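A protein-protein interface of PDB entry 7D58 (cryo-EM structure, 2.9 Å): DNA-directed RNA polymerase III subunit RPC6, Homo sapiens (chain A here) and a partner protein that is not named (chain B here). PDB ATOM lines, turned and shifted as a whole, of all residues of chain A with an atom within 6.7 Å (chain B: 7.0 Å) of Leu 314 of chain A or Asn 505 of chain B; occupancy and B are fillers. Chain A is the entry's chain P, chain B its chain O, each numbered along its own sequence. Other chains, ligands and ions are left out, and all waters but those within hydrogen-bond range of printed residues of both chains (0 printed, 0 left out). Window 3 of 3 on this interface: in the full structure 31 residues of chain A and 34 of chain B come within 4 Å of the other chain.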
ATOM      1  N   TYR A 309     -16.736 -15.439 -22.681  1.00  0.00           N
ATOM      2  CA  TYR A 309     -16.555 -15.181 -24.107  1.00  0.00           C
ATOM      3  C   TYR A 309     -17.893 -15.150 -24.836  1.00  0.00           C
ATOM      4  O   TYR A 309     -18.117 -14.299 -25.705  1.00  0.00           O
ATOM      5  CB  TYR A 309     -15.634 -16.235 -24.719  1.00  0.00           C
ATOM      6  CG  TYR A 309     -14.334 -16.421 -23.975  1.00  0.00           C
ATOM      7  CD1 TYR A 309     -13.311 -15.489 -24.082  1.00  0.00           C
ATOM      8  CD2 TYR A 309     -14.128 -17.532 -23.167  1.00  0.00           C
ATOM      9  CE1 TYR A 309     -12.119 -15.656 -23.403  1.00  0.00           C
ATOM     10  CE2 TYR A 309     -12.942 -17.707 -22.485  1.00  0.00           C
ATOM     11  CZ  TYR A 309     -11.943 -16.768 -22.606  1.00  0.00           C
ATOM     12  OH  TYR A 309     -10.762 -16.945 -21.926  1.00  0.00           O
ATOM     13  N   MET A 310     -18.794 -16.075 -24.498  1.00  0.00           N
ATOM     14  CA  MET A 310     -20.109 -16.107 -25.131  1.00  0.00           C
ATOM     15  C   MET A 310     -20.877 -14.818 -24.859  1.00  0.00           C
ATOM     16  O   MET A 310     -21.486 -14.235 -25.763  1.00  0.00           O
ATOM     17  CB  MET A 310     -20.898 -17.322 -24.637  1.00  0.00           C
ATOM     18  CG  MET A 310     -20.340 -18.663 -25.090  1.00  0.00           C
ATOM     19  SD  MET A 310     -20.318 -18.858 -26.881  1.00  0.00           S
ATOM     20  CE  MET A 310     -22.069 -18.854 -27.250  1.00  0.00           C
ATOM     21  N   THR A 311     -20.851 -14.354 -23.608  1.00  0.00           N
ATOM     22  CA  THR A 311     -21.552 -13.125 -23.252  1.00  0.00           C
ATOM     23  C   THR A 311     -20.933 -11.918 -23.950  1.00  0.00           C
ATOM     24  O   THR A 311     -21.646 -11.033 -24.440  1.00  0.00           O
ATOM     25  CB  THR A 311     -21.538 -12.938 -21.733  1.00  0.00           C
ATOM     26  OG1 THR A 311     -22.284 -13.994 -21.114  1.00  0.00           O
ATOM     27  CG2 THR A 311     -22.158 -11.601 -21.351  1.00  0.00           C
ATOM     28  N   GLU A 312     -19.601 -11.867 -24.005  1.00  0.00           N
ATOM     29  CA  GLU A 312     -18.927 -10.740 -24.646  1.00  0.00           C
ATOM     30  C   GLU A 312     -19.177 -10.735 -26.149  1.00  0.00           C
ATOM     31  O   GLU A 312     -19.170  -9.678 -26.789  1.00  0.00           O
ATOM     32  CB  GLU A 312     -17.429 -10.785 -24.343  1.00  0.00           C
ATOM     33  CG  GLU A 312     -17.061 -10.212 -22.983  1.00  0.00           C
ATOM     34  CD  GLU A 312     -15.605  -9.797 -22.898  1.00  0.00           C
ATOM     35  OE1 GLU A 312     -14.809 -10.236 -23.754  1.00  0.00           O
ATOM     36  OE2 GLU A 312     -15.257  -9.033 -21.973  1.00  0.00           O
ATOM     37  N   TRP A 313     -19.395 -11.915 -26.734  1.00  0.00           N
ATOM     38  CA  TRP A 313     -19.746 -11.985 -28.148  1.00  0.00           C
ATOM     39  C   TRP A 313     -21.196 -11.571 -28.372  1.00  0.00           C
ATOM     40  O   TRP A 313     -21.523 -10.918 -29.369  1.00  0.00           O
ATOM     41  CB  TRP A 313     -19.502 -13.399 -28.678  1.00  0.00           C
ATOM     42  CG  TRP A 313     -19.643 -13.511 -30.164  1.00  0.00           C
ATOM     43  CD1 TRP A 313     -18.953 -12.808 -31.108  1.00  0.00           C
ATOM     44  CD2 TRP A 313     -20.537 -14.373 -30.879  1.00  0.00           C
ATOM     45  NE1 TRP A 313     -19.359 -13.180 -32.367  1.00  0.00           N
ATOM     46  CE2 TRP A 313     -20.330 -14.140 -32.253  1.00  0.00           C
ATOM     47  CE3 TRP A 313     -21.489 -15.320 -30.491  1.00  0.00           C
ATOM     48  CZ2 TRP A 313     -21.043 -14.819 -33.240  1.00  0.00           C
ATOM     49  CZ3 TRP A 313     -22.194 -15.992 -31.471  1.00  0.00           C
ATOM     50  CH2 TRP A 313     -21.967 -15.740 -32.830  1.00  0.00           C
ATOM     51  N   LEU A 314     -22.081 -11.950 -27.448  1.00  0.00           N
ATOM     52  CA  LEU A 314     -23.499 -11.635 -27.605  1.00  0.00           C
ATOM     53  C   LEU A 314     -23.761 -10.144 -27.422  1.00  0.00           C
ATOM     54  O   LEU A 314     -24.595  -9.559 -28.122  1.00  0.00           O
ATOM     55  CB  LEU A 314     -24.331 -12.454 -26.616  1.00  0.00           C
ATOM     56  CG  LEU A 314     -24.499 -13.942 -26.932  1.00  0.00           C
ATOM     57  CD1 LEU A 314     -25.388 -14.614 -25.895  1.00  0.00           C
ATOM     58  CD2 LEU A 314     -25.058 -14.138 -28.333  1.00  0.00           C
ATOM     59  N   GLU A 315     -23.061  -9.513 -26.476  1.00  0.00           N
ATOM     60  CA  GLU A 315     -23.300  -8.100 -26.192  1.00  0.00           C
ATOM     61  C   GLU A 315     -22.883  -7.221 -27.368  1.00  0.00           C
ATOM     62  O   GLU A 315     -23.480  -6.168 -27.616  1.00  0.00           O
ATOM     63  CB  GLU A 315     -22.566  -7.687 -24.912  1.00  0.00           C
ATOM     64  CG  GLU A 315     -21.055  -7.850 -24.957  1.00  0.00           C
ATOM     65  CD  GLU A 315     -20.339  -6.590 -25.407  1.00  0.00           C
ATOM     66  OE1 GLU A 315     -20.909  -5.490 -25.246  1.00  0.00           O
ATOM     67  OE2 GLU A 315     -19.207  -6.701 -25.921  1.00  0.00           O
ATOM     68  N   PHE A 316     -21.858  -7.640 -28.101  1.00  0.00           N
ATOM     69  CA  PHE A 316     -21.373  -6.870 -29.241  1.00  0.00           C
ATOM     70  C   PHE A 316     -22.215  -7.147 -30.481  1.00  0.00           C
ATOM     71  O   PHE A 316     -22.952  -6.279 -30.948  1.00  0.00           O
ATOM     72  CB  PHE A 316     -19.901  -7.184 -29.519  1.00  0.00           C
ATOM     73  CG  PHE A 316     -19.274  -6.289 -30.549  1.00  0.00           C
ATOM     74  CD1 PHE A 316     -18.756  -5.054 -30.191  1.00  0.00           C
ATOM     75  CD2 PHE A 316     -19.196  -6.682 -31.875  1.00  0.00           C
ATOM     76  CE1 PHE A 316     -18.177  -4.228 -31.135  1.00  0.00           C
ATOM     77  CE2 PHE A 316     -18.617  -5.860 -32.824  1.00  0.00           C
ATOM     78  CZ  PHE A 316     -18.108  -4.630 -32.453  1.00  0.00           C
ATOM     79  N   ARG B 449     -26.271 -22.789 -25.556  1.00  0.00           N
ATOM     80  CA  ARG B 449     -26.366 -21.379 -25.192  1.00  0.00           C
ATOM     81  C   ARG B 449     -27.637 -20.745 -25.743  1.00  0.00           C
ATOM     82  O   ARG B 449     -28.237 -19.889 -25.082  1.00  0.00           O
ATOM     83  CB  ARG B 449     -25.134 -20.622 -25.685  1.00  0.00           C
ATOM     84  CG  ARG B 449     -25.155 -19.133 -25.375  1.00  0.00           C
ATOM     85  CD  ARG B 449     -25.147 -18.880 -23.878  1.00  0.00           C
ATOM     86  NE  ARG B 449     -25.146 -17.455 -23.561  1.00  0.00           N
ATOM     87  CZ  ARG B 449     -25.308 -16.963 -22.337  1.00  0.00           C
ATOM     88  NH1 ARG B 449     -25.486 -17.782 -21.309  1.00  0.00           N
ATOM     89  NH2 ARG B 449     -25.293 -15.651 -22.140  1.00  0.00           N
ATOM     90  N   ARG B 450     -28.066 -21.152 -26.939  1.00  0.00           N
ATOM     91  CA  ARG B 450     -29.306 -20.623 -27.496  1.00  0.00           C
ATOM     92  C   ARG B 450     -30.526 -21.109 -26.725  1.00  0.00           C
ATOM     93  O   ARG B 450     -31.470 -20.339 -26.522  1.00  0.00           O
ATOM     94  CB  ARG B 450     -29.425 -21.008 -28.973  1.00  0.00           C
ATOM     95  CG  ARG B 450     -30.603 -20.370 -29.699  1.00  0.00           C
ATOM     96  CD  ARG B 450     -31.762 -21.345 -29.847  1.00  0.00           C
ATOM     97  NE  ARG B 450     -31.410 -22.487 -30.685  1.00  0.00           N
ATOM     98  CZ  ARG B 450     -32.278 -23.401 -31.105  1.00  0.00           C
ATOM     99  NH1 ARG B 450     -33.557 -23.311 -30.763  1.00  0.00           N
ATOM    100  NH2 ARG B 450     -31.870 -24.408 -31.866  1.00  0.00           N
ATOM    101  N   GLU B 453     -30.928 -19.341 -22.663  1.00  0.00           N
ATOM    102  CA  GLU B 453     -31.469 -18.026 -22.340  1.00  0.00           C
ATOM    103  C   GLU B 453     -32.988 -17.970 -22.460  1.00  0.00           C
ATOM    104  O   GLU B 453     -33.607 -17.024 -21.959  1.00  0.00           O
ATOM    105  CB  GLU B 453     -30.840 -16.964 -23.243  1.00  0.00           C
ATOM    106  CG  GLU B 453     -29.379 -16.673 -22.937  1.00  0.00           C
ATOM    107  CD  GLU B 453     -29.193 -15.938 -21.624  1.00  0.00           C
ATOM    108  OE1 GLU B 453     -30.069 -15.121 -21.270  1.00  0.00           O
ATOM    109  OE2 GLU B 453     -28.172 -16.176 -20.948  1.00  0.00           O
ATOM    110  N   GLN B 498     -35.654  -6.928 -22.703  1.00  0.00           N
ATOM    111  CA  GLN B 498     -35.132  -8.291 -22.688  1.00  0.00           C
ATOM    112  C   GLN B 498     -35.323  -8.969 -24.040  1.00  0.00           C
ATOM    113  O   GLN B 498     -34.409  -9.626 -24.550  1.00  0.00           O
ATOM    114  CB  GLN B 498     -35.801  -9.106 -21.578  1.00  0.00           C
ATOM    115  CG  GLN B 498     -35.363  -8.720 -20.178  1.00  0.00           C
ATOM    116  CD  GLN B 498     -33.899  -9.020 -19.921  1.00  0.00           C
ATOM    117  OE1 GLN B 498     -33.374 -10.039 -20.371  1.00  0.00           O
ATOM    118  NE2 GLN B 498     -33.231  -8.130 -19.197  1.00  0.00           N
ATOM    119  N   LEU B 499     -36.512  -8.820 -24.631  1.00  0.00           N
ATOM    120  CA  LEU B 499     -36.763  -9.398 -25.947  1.00  0.00           C
ATOM    121  C   LEU B 499     -35.841  -8.787 -26.993  1.00  0.00           C
ATOM    122  O   LEU B 499     -35.387  -9.478 -27.915  1.00  0.00           O
ATOM    123  CB  LEU B 499     -38.226  -9.191 -26.342  1.00  0.00           C
ATOM    124  CG  LEU B 499     -39.278  -9.354 -25.241  1.00  0.00           C
ATOM    125  CD1 LEU B 499     -40.665  -9.051 -25.783  1.00  0.00           C
ATOM    126  CD2 LEU B 499     -39.232 -10.750 -24.640  1.00  0.00           C
ATOM    127  N   GLU B 500     -35.546  -7.492 -26.856  1.00  0.00           N
ATOM    128  CA  GLU B 500     -34.689  -6.802 -27.814  1.00  0.00           C
ATOM    129  C   GLU B 500     -33.319  -7.462 -27.907  1.00  0.00           C
ATOM    130  O   GLU B 500     -32.775  -7.642 -29.001  1.00  0.00           O
ATOM    131  CB  GLU B 500     -34.548  -5.331 -27.412  1.00  0.00           C
ATOM    132  CG  GLU B 500     -35.844  -4.533 -27.468  1.00  0.00           C
ATOM    133  CD  GLU B 500     -35.662  -3.103 -26.993  1.00  0.00           C
ATOM    134  OE1 GLU B 500     -34.551  -2.776 -26.523  1.00  0.00           O
ATOM    135  OE2 GLU B 500     -36.624  -2.310 -27.078  1.00  0.00           O
ATOM    136  N   THR B 501     -32.753  -7.850 -26.761  1.00  0.00           N
ATOM    137  CA  THR B 501     -31.443  -8.493 -26.766  1.00  0.00           C
ATOM    138  C   THR B 501     -31.559  -9.983 -27.071  1.00  0.00           C
ATOM    139  O   THR B 501     -30.667 -10.567 -27.700  1.00  0.00           O
ATOM    140  CB  THR B 501     -30.734  -8.264 -25.431  1.00  0.00           C
ATOM    141  OG1 THR B 501     -31.553  -8.747 -24.357  1.00  0.00           O
ATOM    142  CG2 THR B 501     -30.449  -6.779 -25.222  1.00  0.00           C
ATOM    143  N   LEU B 502     -32.650 -10.618 -26.634  1.00  0.00           N
ATOM    144  CA  LEU B 502     -32.807 -12.054 -26.843  1.00  0.00           C
ATOM    145  C   LEU B 502     -32.941 -12.391 -28.322  1.00  0.00           C
ATOM    146  O   LEU B 502     -32.360 -13.370 -28.804  1.00  0.00           O
ATOM    147  CB  LEU B 502     -34.017 -12.571 -26.063  1.00  0.00           C
ATOM    148  CG  LEU B 502     -33.795 -12.792 -24.565  1.00  0.00           C
ATOM    149  CD1 LEU B 502     -35.111 -13.090 -23.859  1.00  0.00           C
ATOM    150  CD2 LEU B 502     -32.787 -13.907 -24.325  1.00  0.00           C
ATOM    151  N   LYS B 503     -33.708 -11.585 -29.062  1.00  0.00           N
ATOM    152  CA  LYS B 503     -33.859 -11.826 -30.494  1.00  0.00           C
ATOM    153  C   LYS B 503     -32.523 -11.688 -31.213  1.00  0.00           C
ATOM    154  O   LYS B 503     -32.174 -12.510 -32.068  1.00  0.00           O
ATOM    155  CB  LYS B 503     -34.894 -10.864 -31.083  1.00  0.00           C
ATOM    156  CG  LYS B 503     -36.326 -11.106 -30.615  1.00  0.00           C
ATOM    157  CD  LYS B 503     -36.928 -12.348 -31.256  1.00  0.00           C
ATOM    158  CE  LYS B 503     -37.013 -13.502 -30.269  1.00  0.00           C
ATOM    159  NZ  LYS B 503     -37.673 -14.697 -30.864  1.00  0.00           N
ATOM    160  N   ARG B 504     -31.753 -10.654 -30.860  1.00  0.00           N
ATOM    161  CA  ARG B 504     -30.449 -10.449 -31.483  1.00  0.00           C
ATOM    162  C   ARG B 504     -29.500 -11.597 -31.163  1.00  0.00           C
ATOM    163  O   ARG B 504     -28.764 -12.069 -32.036  1.00  0.00           O
ATOM    164  CB  ARG B 504     -29.856  -9.115 -31.027  1.00  0.00           C
ATOM    165  CG  ARG B 504     -30.650  -7.898 -31.473  1.00  0.00           C
ATOM    166  CD  ARG B 504     -30.271  -6.668 -30.667  1.00  0.00           C
ATOM    167  NE  ARG B 504     -28.867  -6.308 -30.839  1.00  0.00           N
ATOM    168  CZ  ARG B 504     -28.280  -5.290 -30.219  1.00  0.00           C
ATOM    169  NH1 ARG B 504     -28.975  -4.530 -29.385  1.00  0.00           N
ATOM    170  NH2 ARG B 504     -26.997  -5.034 -30.434  1.00  0.00           N
ATOM    171  N   ASN B 505     -29.502 -12.059 -29.911  1.00  0.00           N
ATOM    172  CA  ASN B 505     -28.615 -13.154 -29.525  1.00  0.00           C
ATOM    173  C   ASN B 505     -28.995 -14.445 -30.239  1.00  0.00           C
ATOM    174  O   ASN B 505     -28.125 -15.188 -30.712  1.00  0.00           O
ATOM    175  CB  ASN B 505     -28.646 -13.342 -28.008  1.00  0.00           C
ATOM    176  CG  ASN B 505     -28.105 -12.141 -27.260  1.00  0.00           C
ATOM    177  OD1 ASN B 505     -27.277 -11.392 -27.781  1.00  0.00           O
ATOM    178  ND2 ASN B 505     -28.570 -11.948 -26.031  1.00  0.00           N
ATOM    179  N   VAL B 506     -30.298 -14.728 -30.330  1.00  0.00           N
ATOM    180  CA  VAL B 506     -30.757 -15.935 -31.016  1.00  0.00           C
ATOM    181  C   VAL B 506     -30.384 -15.872 -32.492  1.00  0.00           C
ATOM    182  O   VAL B 506     -29.941 -16.862 -33.085  1.00  0.00           O
ATOM    183  CB  VAL B 506     -32.273 -16.121 -30.824  1.00  0.00           C
ATOM    184  CG1 VAL B 506     -32.825 -17.126 -31.825  1.00  0.00           C
ATOM    185  CG2 VAL B 506     -32.573 -16.566 -29.400  1.00  0.00           C
ATOM    186  N   ASN B 507     -30.541 -14.693 -33.100  1.00  0.00           N
ATOM    187  CA  ASN B 507     -30.171 -14.526 -34.502  1.00  0.00           C
ATOM    188  C   ASN B 507     -28.676 -14.736 -34.705  1.00  0.00           C
ATOM    189  O   ASN B 507     -28.255 -15.424 -35.642  1.00  0.00           O
ATOM    190  CB  ASN B 507     -30.593 -13.139 -34.991  1.00  0.00           C
ATOM    191  CG  ASN B 507     -32.086 -13.033 -35.223  1.00  0.00           C
ATOM    192  OD1 ASN B 507     -32.859 -13.875 -34.764  1.00  0.00           O
ATOM    193  ND2 ASN B 507     -32.501 -11.995 -35.939  1.00  0.00           N
ATOM    194  N   LYS B 508     -27.856 -14.146 -33.831  1.00  0.00           N
ATOM    195  CA  LYS B 508     -26.408 -14.299 -33.933  1.00  0.00           C
ATOM    196  C   LYS B 508     -25.998 -15.762 -33.814  1.00  0.00           C
ATOM    197  O   LYS B 508     -25.176 -16.256 -34.595  1.00  0.00           O
ATOM    198  CB  LYS B 508     -25.720 -13.459 -32.855  1.00  0.00           C
ATOM    199  CG  LYS B 508     -25.137 -12.149 -33.358  1.00  0.00           C
ATOM    200  CD  LYS B 508     -23.961 -11.710 -32.500  1.00  0.00           C
ATOM    201  CE  LYS B 508     -23.200 -10.564 -33.144  1.00  0.00           C
ATOM    202  NZ  LYS B 508     -21.938 -10.260 -32.415  1.00  0.00           N
ATOM    203  N   LEU B 509     -26.565 -16.473 -32.837  1.00  0.00           N
ATOM    204  CA  LEU B 509     -26.214 -17.877 -32.653  1.00  0.00           C
ATOM    205  C   LEU B 509     -26.680 -18.737 -33.822  1.00  0.00           C
ATOM    206  O   LEU B 509     -25.927 -19.597 -34.297  1.00  0.00           O
ATOM    207  CB  LEU B 509     -26.794 -18.395 -31.338  1.00  0.00           C
ATOM    208  CG  LEU B 509     -26.203 -17.757 -30.079  1.00  0.00           C
ATOM    209  CD1 LEU B 509     -26.966 -18.190 -28.839  1.00  0.00           C
ATOM    210  CD2 LEU B 509     -24.726 -18.098 -29.948  1.00  0.00           C
ATOM    211  N   ASP B 510     -27.902 -18.513 -34.314  1.00  0.00           N
ATOM    212  CA  ASP B 510     -28.406 -19.315 -35.421  1.00  0.00           C
ATOM    213  C   ASP B 510     -27.687 -18.994 -36.726  1.00  0.00           C
ATOM    214  O   ASP B 510     -27.647 -19.836 -37.630  1.00  0.00           O
ATOM    215  CB  ASP B 510     -29.913 -19.107 -35.576  1.00  0.00           C
ATOM    216  CG  ASP B 510     -30.715 -19.906 -34.567  1.00  0.00           C
ATOM    217  OD1 ASP B 510     -30.309 -21.044 -34.249  1.00  0.00           O
ATOM    218  OD2 ASP B 510     -31.750 -19.394 -34.092  1.00  0.00           O
ATOM    219  N   ALA B 511     -27.119 -17.794 -36.847  1.00  0.00           N
ATOM    220  CA  ALA B 511     -26.323 -17.432 -38.010  1.00  0.00           C
ATOM    221  C   ALA B 511     -24.904 -17.973 -37.935  1.00  0.00           C
ATOM    222  O   ALA B 511     -24.341 -18.342 -38.970  1.00  0.00           O
ATOM    223  CB  ALA B 511     -26.289 -15.910 -38.177  1.00  0.00           C
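O of Thr 501 of chain B sits at hydrogen-bond distance from ND2 of Asn 505 of chain B (3.0 Å). NH1 of Arg 449 of chain B lies within salt-bridge range of OE2 of Glu 453 of chain B (3.2 Å).
The side-chain amino group of Lys 508 of chain B sits at hydrogen-bond distance from the backbone carbonyl oxygen of Trp 313 of chain A (3.1 Å). OD1 of Asn 505 of chain B sits close to O of Leu 314 of chain A (3.3 Å).
Hydrophobic or aromatic side chains of chain A that line the printed part of chain B: Met 310, Trp 313 and Leu 314. Of the 17 printed residues of chain B, 4 touch a printed residue of chain A. Among the printed residues, 8 pairs touch across the chains.
Of the printed residues of chain B, Leu 314 of chain A touches Arg 449 (3.7 Å) and Asn 505 (3.3 Å). Of the printed residues of chain B, Trp 313 of chain A touches Lys 508 (3.1 Å) and Leu 509 (3.6 Å). Of the printed residues of chain A, Arg 449 of chain B touches Met 310 (3.6 Å), Thr 311 (3.6 Å) and Leu 314 (3.7 Å). Printed residues of chain B within 4 Å of Thr 311 of chain A: Arg 449 (3.6 Å). Of the printed residues of chain B, Phe 316 of chain A touches Lys 508 (3.7 Å). Printed residues of chain A within 4 Å of Leu 509 of chain B: Met 310 (3.9 Å) and Trp 313 (3.6 Å). The nearest residue of chain A that does not touch Asn 505 of chain B is Glu 315 of chain A (4.8 Å). The nearest printed residue of chain B that does not touch Trp 313 of chain A is Asn 505 of chain B (6.0 Å).
Met 310 of chain A touches Arg 449 of chain B (CE to CG, 3.6 Å). Leu 509 of chain B touches Met 310 of chain A. Arg 449 of chain B touches Thr 311 of chain A (NH2 to OG1, 3.6 Å). CZ3 of Trp 313 of chain A touches CD2 of Leu 509 of chain B (3.6 Å). Leu 314 of chain A touches Arg 449 of chain B. NZ of Lys 508 of chain B touches C of Phe 316 of chain A (3.7 Å).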
